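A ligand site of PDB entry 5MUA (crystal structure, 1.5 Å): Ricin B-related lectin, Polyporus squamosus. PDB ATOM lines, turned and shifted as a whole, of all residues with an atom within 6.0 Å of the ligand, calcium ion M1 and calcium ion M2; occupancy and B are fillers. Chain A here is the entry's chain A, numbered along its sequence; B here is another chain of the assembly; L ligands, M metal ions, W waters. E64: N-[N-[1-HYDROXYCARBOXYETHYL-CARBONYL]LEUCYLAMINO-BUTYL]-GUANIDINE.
Calcium ion M1 is bound by the backbone carbonyl oxygen (O) of Glu 204 (2.3 Å), the side-chain carboxylate (OD1) of Asp 207 (2.3 Å), water W4 (2.4 Å), the side-chain carboxylate (OD2) of Asp 210 (2.4 Å), the side-chain carboxylate (OD1) of Asp 209 (2.5 Å), the side-chain carboxylate (OD2) of Asp 176 of chain B (2.5 Å) and the side-chain carboxylate (OD1) of Asp 176 of chain B (2.6 Å).
Within 4 Å of calcium ion M1: Glu 204, Asp 207, Asp 209, Asp 210 and Asp 176 of chain B. Along chain A the residues within 4 Å of calcium ion M1 span positions 204 to 210.
Water W3 lies within hydrogen-bond range of an oxygen (O1) of the ligand (2.7 Å) and the side-chain amide nitrogen (NE2) of Gln 268 (2.9 Å). Water W1 bridges a nitrogen (N4) of the ligand and the backbone NH (N) of Leu 174 of chain B. Water W5 bridges OH of Tyr 282 (2.8 Å) and N3 of the ligand (3.4 Å).
Within 4 Å of calcium ion M2: Asp 207, Asp 209, Ser 175 of chain B and Asp 176 of chain B. Along chain A the residues within 4 Å of calcium ion M2 span positions 207 to 209.
Calcium ion M2 is bound by O4 of the ligand (2.2 Å), OD1 of Asp 176 of chain B (2.3 Å), OD2 of Asp 209 (2.3 Å), O of Ser 175 of chain B (2.4 Å), water W2 (2.4 Å) and OD2 of Asp 207 (2.5 Å). Calcium ion M2 has six donor atoms within binding distance.
N of Ala 249 sits at hydrogen-bond distance from SG of Cys 208 (3.5 Å). The side-chain carboxylate (OE1) of Glu 204 sits at hydrogen-bond distance from the backbone NH (N) of Gly 177 of chain B (2.8 Å). The backbone NH (N) of His 248 lies within hydrogen-bond range of the backbone carbonyl oxygen (O) of Gly 241, 2.9 Å away. N of Tyr 282 lies within hydrogen-bond range of O of Phe 240 (2.7 Å).
Phe 240 touches the ligand. N of Ala 249 touches C10 of the ligand (3.7 Å). OH of Tyr 282 touches C10 of the ligand, at 3.6 Å. Leu 174 of chain B touches the ligand. Hydrophobic or aromatic side chains within 4 Å of the ligand: Trp 201, Phe 240, Ala 247, His 248 and Leu 174 of chain B. Within 4 Å of the ligand: Trp 201, Asp 207, Cys 208, Asp 209, Phe 240, Ala 247, His 248, Ala 249, Tyr 282, Leu 174 of chain B and Ser 175 of chain B. The nearest printed residue that does not touch the ligand is Gln 268 (4.3 Å).
N of Cys 208 sits at hydrogen-bond distance from O2 of the ligand (2.9 Å). A carbon (C2) of the ligand is covalently linked to the side-chain sulfur of Cys 208. NE1 of Trp 201 lies within hydrogen-bond range of O2 of the ligand (2.7 Å). A ring nitrogen (ND1) of His 248 lies within hydrogen-bond range of an oxygen (O1) of the ligand. O of Ala 247 is in hydrogen-bond range of N1 of the ligand, at 3.4 Å.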
ATOM      1  N   TRP A 201       4.128 -22.526  -7.762  1.00  0.00           N
ATOM      2  CA  TRP A 201       3.779 -22.733  -6.363  1.00  0.00           C
ATOM      3  C   TRP A 201       3.983 -21.406  -5.629  1.00  0.00           C
ATOM      4  O   TRP A 201       5.010 -20.745  -5.805  1.00  0.00           O
ATOM      5  CB  TRP A 201       4.698 -23.792  -5.737  1.00  0.00           C
ATOM      6  CG  TRP A 201       4.401 -24.107  -4.304  1.00  0.00           C
ATOM      7  CD1 TRP A 201       3.647 -25.127  -3.826  1.00  0.00           C
ATOM      8  CD2 TRP A 201       4.883 -23.404  -3.138  1.00  0.00           C
ATOM      9  NE1 TRP A 201       3.619 -25.120  -2.459  1.00  0.00           N
ATOM     10  CE2 TRP A 201       4.356 -24.055  -2.010  1.00  0.00           C
ATOM     11  CE3 TRP A 201       5.744 -22.325  -2.948  1.00  0.00           C
ATOM     12  CZ2 TRP A 201       4.598 -23.625  -0.707  1.00  0.00           C
ATOM     13  CZ3 TRP A 201       5.986 -21.875  -1.661  1.00  0.00           C
ATOM     14  CH2 TRP A 201       5.444 -22.558  -0.553  1.00  0.00           C
ATOM     15  N   GLU A 204       0.768 -20.338   0.559  1.00  0.00           N
ATOM     16  CA  GLU A 204      -0.618 -20.176   0.988  1.00  0.00           C
ATOM     17  C   GLU A 204      -1.619 -19.855  -0.119  1.00  0.00           C
ATOM     18  O   GLU A 204      -2.718 -20.473  -0.169  1.00  0.00           O
ATOM     19  CB  GLU A 204      -0.821 -19.241   2.180  1.00  0.00           C
ATOM     20  CG  GLU A 204       0.087 -19.563   3.341  1.00  0.00           C
ATOM     21  CD  GLU A 204      -0.617 -19.643   4.640  1.00  0.00           C
ATOM     22  OE1 GLU A 204      -0.370 -20.615   5.302  1.00  0.00           O
ATOM     23  OE2 GLU A 204      -1.392 -18.791   5.040  1.00  0.00           O
ATOM     24  N   ILE A 205      -1.277 -18.863  -0.901  1.00  0.00           N
ATOM     25  CA  ILE A 205      -2.128 -18.321  -1.935  1.00  0.00           C
ATOM     26  C   ILE A 205      -2.309 -19.331  -3.096  1.00  0.00           C
ATOM     27  O   ILE A 205      -3.348 -19.348  -3.710  1.00  0.00           O
ATOM     28  CB  ILE A 205      -1.638 -16.980  -2.455  1.00  0.00           C
ATOM     29  CG1 ILE A 205      -2.728 -16.244  -3.235  1.00  0.00           C
ATOM     30  CG2 ILE A 205      -0.340 -17.034  -3.206  1.00  0.00           C
ATOM     31  CD1 ILE A 205      -3.947 -15.822  -2.446  1.00  0.00           C
ATOM     32  N   PHE A 206      -1.309 -20.152  -3.369  1.00  0.00           N
ATOM     33  CA  PHE A 206      -1.563 -21.270  -4.328  1.00  0.00           C
ATOM     34  C   PHE A 206      -0.535 -22.338  -4.085  1.00  0.00           C
ATOM     35  O   PHE A 206       0.437 -22.441  -4.789  1.00  0.00           O
ATOM     36  CB  PHE A 206      -1.539 -20.784  -5.756  1.00  0.00           C
ATOM     37  CG  PHE A 206      -2.381 -21.623  -6.635  1.00  0.00           C
ATOM     38  CD1 PHE A 206      -3.763 -21.452  -6.652  1.00  0.00           C
ATOM     39  CD2 PHE A 206      -1.834 -22.652  -7.314  1.00  0.00           C
ATOM     40  CE1 PHE A 206      -4.572 -22.272  -7.472  1.00  0.00           C
ATOM     41  CE2 PHE A 206      -2.621 -23.474  -8.136  1.00  0.00           C
ATOM     42  CZ  PHE A 206      -3.975 -23.281  -8.225  1.00  0.00           C
ATOM     43  N   ASP A 207      -0.759 -23.055  -3.017  1.00  0.00           N
ATOM     44  CA  ASP A 207       0.173 -24.065  -2.530  1.00  0.00           C
ATOM     45  C   ASP A 207      -0.534 -25.432  -2.640  1.00  0.00           C
ATOM     46  O   ASP A 207      -1.517 -25.540  -3.402  1.00  0.00           O
ATOM     47  CB  ASP A 207       0.740 -23.703  -1.184  1.00  0.00           C
ATOM     48  CG  ASP A 207      -0.329 -23.572  -0.118  1.00  0.00           C
ATOM     49  OD1 ASP A 207      -1.555 -23.406  -0.411  1.00  0.00           O
ATOM     50  OD2 ASP A 207       0.069 -23.613   1.050  1.00  0.00           O
ATOM     51  N   CYS A 208      -0.006 -26.452  -1.981  1.00  0.00           N
ATOM     52  CA  CYS A 208      -0.392 -27.823  -2.295  1.00  0.00           C
ATOM     53  C   CYS A 208      -1.915 -28.036  -2.194  1.00  0.00           C
ATOM     54  O   CYS A 208      -2.487 -28.659  -3.115  1.00  0.00           O
ATOM     55  CB  CYS A 208       0.338 -28.820  -1.404  1.00  0.00           C
ATOM     56  SG  CYS A 208       0.071 -28.510   0.375  1.00  0.00           S
ATOM     57  N   ASP A 209      -2.564 -27.502  -1.135  1.00  0.00           N
ATOM     58  CA  ASP A 209      -4.001 -27.650  -0.990  1.00  0.00           C
ATOM     59  C   ASP A 209      -4.765 -27.132  -2.198  1.00  0.00           C
ATOM     60  O   ASP A 209      -5.722 -27.701  -2.602  1.00  0.00           O
ATOM     61  CB  ASP A 209      -4.488 -27.071   0.316  1.00  0.00           C
ATOM     62  CG  ASP A 209      -4.055 -25.645   0.533  1.00  0.00           C
ATOM     63  OD1 ASP A 209      -4.794 -24.751   0.114  1.00  0.00           O
ATOM     64  OD2 ASP A 209      -2.969 -25.482   1.117  1.00  0.00           O
ATOM     65  N   ASP A 210      -4.288 -26.019  -2.781  1.00  0.00           N
ATOM     66  CA  ASP A 210      -4.884 -25.458  -3.954  1.00  0.00           C
ATOM     67  C   ASP A 210      -4.697 -26.340  -5.176  1.00  0.00           C
ATOM     68  O   ASP A 210      -5.624 -26.519  -5.910  1.00  0.00           O
ATOM     69  CB  ASP A 210      -4.333 -24.063  -4.209  1.00  0.00           C
ATOM     70  CG  ASP A 210      -4.643 -23.146  -3.013  1.00  0.00           C
ATOM     71  OD1 ASP A 210      -5.841 -22.890  -2.778  1.00  0.00           O
ATOM     72  OD2 ASP A 210      -3.740 -22.808  -2.312  1.00  0.00           O
ATOM     73  N   MET A 239      -6.361 -36.011  -0.793  1.00  0.00           N
ATOM     74  CA  MET A 239      -5.836 -36.422   0.488  1.00  0.00           C
ATOM     75  C   MET A 239      -4.996 -35.288   1.074  1.00  0.00           C
ATOM     76  O   MET A 239      -4.329 -34.557   0.306  1.00  0.00           O
ATOM     77  CB  MET A 239      -4.964 -37.637   0.392  1.00  0.00           C
ATOM     78  CG  MET A 239      -5.695 -38.921   0.605  1.00  0.00           C
ATOM     79  SD  MET A 239      -4.540 -40.272   0.134  1.00  0.00           S
ATOM     80  CE  MET A 239      -5.759 -41.560   0.365  1.00  0.00           C
ATOM     81  N   PHE A 240      -5.064 -35.195   2.380  1.00  0.00           N
ATOM     82  CA  PHE A 240      -4.061 -34.494   3.185  1.00  0.00           C
ATOM     83  C   PHE A 240      -3.315 -35.560   3.944  1.00  0.00           C
ATOM     84  O   PHE A 240      -3.934 -36.438   4.607  1.00  0.00           O
ATOM     85  CB  PHE A 240      -4.625 -33.477   4.170  1.00  0.00           C
ATOM     86  CG  PHE A 240      -5.294 -32.230   3.540  1.00  0.00           C
ATOM     87  CD1 PHE A 240      -5.356 -31.973   2.182  1.00  0.00           C
ATOM     88  CD2 PHE A 240      -5.734 -31.228   4.385  1.00  0.00           C
ATOM     89  CE1 PHE A 240      -5.906 -30.843   1.647  1.00  0.00           C
ATOM     90  CE2 PHE A 240      -6.337 -30.091   3.853  1.00  0.00           C
ATOM     91  CZ  PHE A 240      -6.428 -29.894   2.489  1.00  0.00           C
ATOM     92  N   GLY A 241      -1.994 -35.429   3.953  1.00  0.00           N
ATOM     93  CA  GLY A 241      -1.157 -36.392   4.705  1.00  0.00           C
ATOM     94  C   GLY A 241       0.077 -35.792   5.281  1.00  0.00           C
ATOM     95  O   GLY A 241       0.438 -34.712   4.904  1.00  0.00           O
ATOM     96  N   GLY A 246       6.941 -32.839   7.124  1.00  0.00           N
ATOM     97  CA  GLY A 246       5.813 -31.935   6.962  1.00  0.00           C
ATOM     98  C   GLY A 246       4.595 -32.610   6.394  1.00  0.00           C
ATOM     99  O   GLY A 246       4.474 -33.855   6.399  1.00  0.00           O
ATOM    100  N   ALA A 247       3.668 -31.782   5.944  1.00  0.00           N
ATOM    101  CA  ALA A 247       2.334 -32.244   5.528  1.00  0.00           C
ATOM    102  C   ALA A 247       2.054 -31.667   4.159  1.00  0.00           C
ATOM    103  O   ALA A 247       2.576 -30.640   3.807  1.00  0.00           O
ATOM    104  CB  ALA A 247       1.272 -31.899   6.517  1.00  0.00           C
ATOM    105  N   HIS A 248       1.218 -32.367   3.382  1.00  0.00           N
ATOM    106  CA  HIS A 248       1.078 -32.112   1.989  1.00  0.00           C
ATOM    107  C   HIS A 248      -0.312 -32.559   1.520  1.00  0.00           C
ATOM    108  O   HIS A 248      -0.829 -33.511   2.051  1.00  0.00           O
ATOM    109  CB  HIS A 248       2.151 -32.946   1.267  1.00  0.00           C
ATOM    110  CG  HIS A 248       2.323 -32.624  -0.183  1.00  0.00           C
ATOM    111  ND1 HIS A 248       2.754 -31.407  -0.644  1.00  0.00           N
ATOM    112  CD2 HIS A 248       2.183 -33.396  -1.287  1.00  0.00           C
ATOM    113  CE1 HIS A 248       2.867 -31.430  -1.945  1.00  0.00           C
ATOM    114  NE2 HIS A 248       2.483 -32.628  -2.369  1.00  0.00           N
ATOM    115  N   ALA A 249      -0.821 -31.864   0.541  1.00  0.00           N
ATOM    116  CA  ALA A 249      -2.043 -32.194  -0.179  1.00  0.00           C
ATOM    117  C   ALA A 249      -1.763 -32.738  -1.526  1.00  0.00           C
ATOM    118  O   ALA A 249      -0.911 -32.267  -2.212  1.00  0.00           O
ATOM    119  CB  ALA A 249      -2.880 -30.985  -0.319  1.00  0.00           C
ATOM    120  N   GLN A 268       0.845 -30.763  -8.823  1.00  0.00           N
ATOM    121  CA  GLN A 268       1.810 -29.674  -9.199  1.00  0.00           C
ATOM    122  C   GLN A 268       2.600 -30.020 -10.417  1.00  0.00           C
ATOM    123  O   GLN A 268       3.014 -29.153 -11.141  1.00  0.00           O
ATOM    124  CB  GLN A 268       2.760 -29.408  -8.035  1.00  0.00           C
ATOM    125  CG  GLN A 268       2.124 -28.675  -6.903  1.00  0.00           C
ATOM    126  CD  GLN A 268       3.121 -28.279  -5.826  1.00  0.00           C
ATOM    127  OE1 GLN A 268       4.159 -27.672  -6.141  1.00  0.00           O
ATOM    128  NE2 GLN A 268       2.840 -28.638  -4.572  1.00  0.00           N
ATOM    129  N   TYR A 279       3.974 -39.889   2.462  1.00  0.00           N
ATOM    130  CA  TYR A 279       2.985 -39.206   3.247  1.00  0.00           C
ATOM    131  C   TYR A 279       2.010 -40.226   3.734  1.00  0.00           C
ATOM    132  O   TYR A 279       1.646 -41.135   2.977  1.00  0.00           O
ATOM    133  CB  TYR A 279       2.289 -38.052   2.456  1.00  0.00           C
ATOM    134  CG  TYR A 279       3.171 -36.843   2.205  1.00  0.00           C
ATOM    135  CD1 TYR A 279       3.451 -35.976   3.237  1.00  0.00           C
ATOM    136  CD2 TYR A 279       3.765 -36.600   0.979  1.00  0.00           C
ATOM    137  CE1 TYR A 279       4.262 -34.864   3.040  1.00  0.00           C
ATOM    138  CE2 TYR A 279       4.639 -35.492   0.749  1.00  0.00           C
ATOM    139  CZ  TYR A 279       4.896 -34.652   1.795  1.00  0.00           C
ATOM    140  OH  TYR A 279       5.693 -33.553   1.669  1.00  0.00           O
ATOM    141  N   TYR A 282      -4.199 -38.330   6.530  1.00  0.00           N
ATOM    142  CA  TYR A 282      -5.129 -38.161   7.652  1.00  0.00           C
ATOM    143  C   TYR A 282      -6.563 -37.769   7.239  1.00  0.00           C
ATOM    144  O   TYR A 282      -7.501 -37.949   8.032  1.00  0.00           O
ATOM    145  CB  TYR A 282      -4.586 -37.258   8.724  1.00  0.00           C
ATOM    146  CG  TYR A 282      -4.277 -35.873   8.310  1.00  0.00           C
ATOM    147  CD1 TYR A 282      -5.292 -34.855   8.263  1.00  0.00           C
ATOM    148  CD2 TYR A 282      -2.978 -35.507   7.953  1.00  0.00           C
ATOM    149  CE1 TYR A 282      -4.980 -33.533   7.880  1.00  0.00           C
ATOM    150  CE2 TYR A 282      -2.667 -34.194   7.565  1.00  0.00           C
ATOM    151  CZ  TYR A 282      -3.659 -33.208   7.550  1.00  0.00           C
ATOM    152  OH  TYR A 282      -3.291 -31.938   7.180  1.00  0.00           O
ATOM    153  N   LEU B 174      -7.837 -27.929   8.126  1.00  0.00           N
ATOM    154  CA  LEU B 174      -7.404 -26.599   7.860  1.00  0.00           C
ATOM    155  C   LEU B 174      -6.298 -26.701   6.812  1.00  0.00           C
ATOM    156  O   LEU B 174      -5.472 -27.627   6.899  1.00  0.00           O
ATOM    157  CB  LEU B 174      -6.845 -26.004   9.201  1.00  0.00           C
ATOM    158  CG  LEU B 174      -5.872 -24.840   9.219  1.00  0.00           C
ATOM    159  CD1 LEU B 174      -6.736 -23.629   8.913  1.00  0.00           C
ATOM    160  CD2 LEU B 174      -5.179 -24.627  10.564  1.00  0.00           C
ATOM    161  N   SER B 175      -6.272 -25.763   5.888  1.00  0.00           N
ATOM    162  CA  SER B 175      -5.363 -25.700   4.767  1.00  0.00           C
ATOM    163  C   SER B 175      -4.191 -24.712   4.877  1.00  0.00           C
ATOM    164  O   SER B 175      -3.107 -25.007   4.430  1.00  0.00           O
ATOM    165  CB  SER B 175      -6.157 -25.395   3.496  1.00  0.00           C
ATOM    166  OG  SER B 175      -7.172 -26.362   3.360  1.00  0.00           O
ATOM    167  N   ASP B 176      -4.462 -23.526   5.429  1.00  0.00           N
ATOM    168  CA  ASP B 176      -3.559 -22.396   5.425  1.00  0.00           C
ATOM    169  C   ASP B 176      -3.539 -21.727   6.784  1.00  0.00           C
ATOM    170  O   ASP B 176      -4.290 -22.089   7.660  1.00  0.00           O
ATOM    171  CB  ASP B 176      -3.950 -21.410   4.336  1.00  0.00           C
ATOM    172  CG  ASP B 176      -3.845 -22.055   2.913  1.00  0.00           C
ATOM    173  OD1 ASP B 176      -2.720 -22.436   2.528  1.00  0.00           O
ATOM    174  OD2 ASP B 176      -4.875 -22.166   2.235  1.00  0.00           O
ATOM    175  N   GLY B 177      -2.613 -20.813   6.940  1.00  0.00           N
ATOM    176  CA  GLY B 177      -2.412 -20.105   8.209  1.00  0.00           C
ATOM    177  C   GLY B 177      -3.092 -18.752   8.370  1.00  0.00           C
ATOM    178  O   GLY B 177      -3.435 -18.390   9.499  1.00  0.00           O
ATOM    179  N   ALA B 233      -4.214 -16.869   2.226  1.00  0.00           N
ATOM    180  CA  ALA B 233      -5.158 -17.559   1.381  1.00  0.00           C
ATOM    181  C   ALA B 233      -6.466 -16.878   1.501  1.00  0.00           C
ATOM    182  O   ALA B 233      -6.664 -16.020   2.364  1.00  0.00           O
ATOM    183  CB  ALA B 233      -5.300 -19.017   1.814  1.00  0.00           C
HETATM  184  C1  E64 L   1       2.691 -27.764   0.012  1.00  0.00           C
HETATM  185  O1  E64 L   1       3.583 -28.623  -0.197  1.00  0.00           O
HETATM  186  O2  E64 L   1       2.517 -26.771  -0.691  1.00  0.00           O
HETATM  187  C2  E64 L   1       1.699 -28.058   1.119  1.00  0.00           C
HETATM  188  C3  E64 L   1       1.558 -26.784   1.960  1.00  0.00           C
HETATM  189  O3  E64 L   1       2.878 -26.705   2.622  1.00  0.00           O
HETATM  190  C4  E64 L   1       0.528 -26.933   3.023  1.00  0.00           C
HETATM  191  O4  E64 L   1      -0.507 -26.306   3.049  1.00  0.00           O
HETATM  192  N1  E64 L   1       0.818 -27.748   3.978  1.00  0.00           N
HETATM  193  C6  E64 L   1       0.091 -28.075   5.189  1.00  0.00           C
HETATM  194  C7  E64 L   1      -0.969 -29.182   5.158  1.00  0.00           C
HETATM  195  C8  E64 L   1      -1.663 -29.476   3.835  1.00  0.00           C
HETATM  196  C9  E64 L   1      -2.862 -28.507   3.875  1.00  0.00           C
HETATM  197  C10 E64 L   1      -2.095 -30.941   3.945  1.00  0.00           C
HETATM  198  C11 E64 L   1       0.667 -27.742   6.584  1.00  0.00           C
HETATM  199  O5  E64 L   1       1.764 -28.283   6.743  1.00  0.00           O
HETATM  200  N2  E64 L   1       0.031 -26.997   7.544  1.00  0.00           N
HETATM  201  C12 E64 L   1      -1.152 -26.130   7.448  1.00  0.00           C
HETATM  202  C13 E64 L   1      -2.516 -26.786   7.512  1.00  0.00           C
HETATM  203  C14 E64 L   1      -2.992 -26.873   8.921  1.00  0.00           C
HETATM  204  C15 E64 L   1      -2.384 -28.029   9.637  1.00  0.00           C
HETATM  205  N3  E64 L   1      -3.413 -28.608  10.432  1.00  0.00           N
HETATM  206  C16 E64 L   1      -3.711 -28.060  11.583  1.00  0.00           C
HETATM  207  N4  E64 L   1      -4.848 -28.338  12.194  1.00  0.00           N
HETATM  208  N5  E64 L   1      -2.885 -27.156  12.069  1.00  0.00           N
HETATM  209 CA    CA M   1      -3.684 -22.562   0.081  1.00  0.00          CA
HETATM  210 CA    CA M   2      -1.581 -24.457   2.692  1.00  0.00          CA
HETATM  211  O   HOH W   1      -6.305 -29.658  10.037  1.00  0.00           O
HETATM  212  O   HOH W   2      -0.193 -23.592   4.457  1.00  0.00           O
HETATM  213  O   HOH W   3       4.878 -28.524  -2.518  1.00  0.00           O
HETATM  214  O   HOH W   4      -5.754 -21.637  -0.539  1.00  0.00           O
HETATM  215  O   HOH W   5      -1.381 -30.809   8.883  1.00  0.00           O
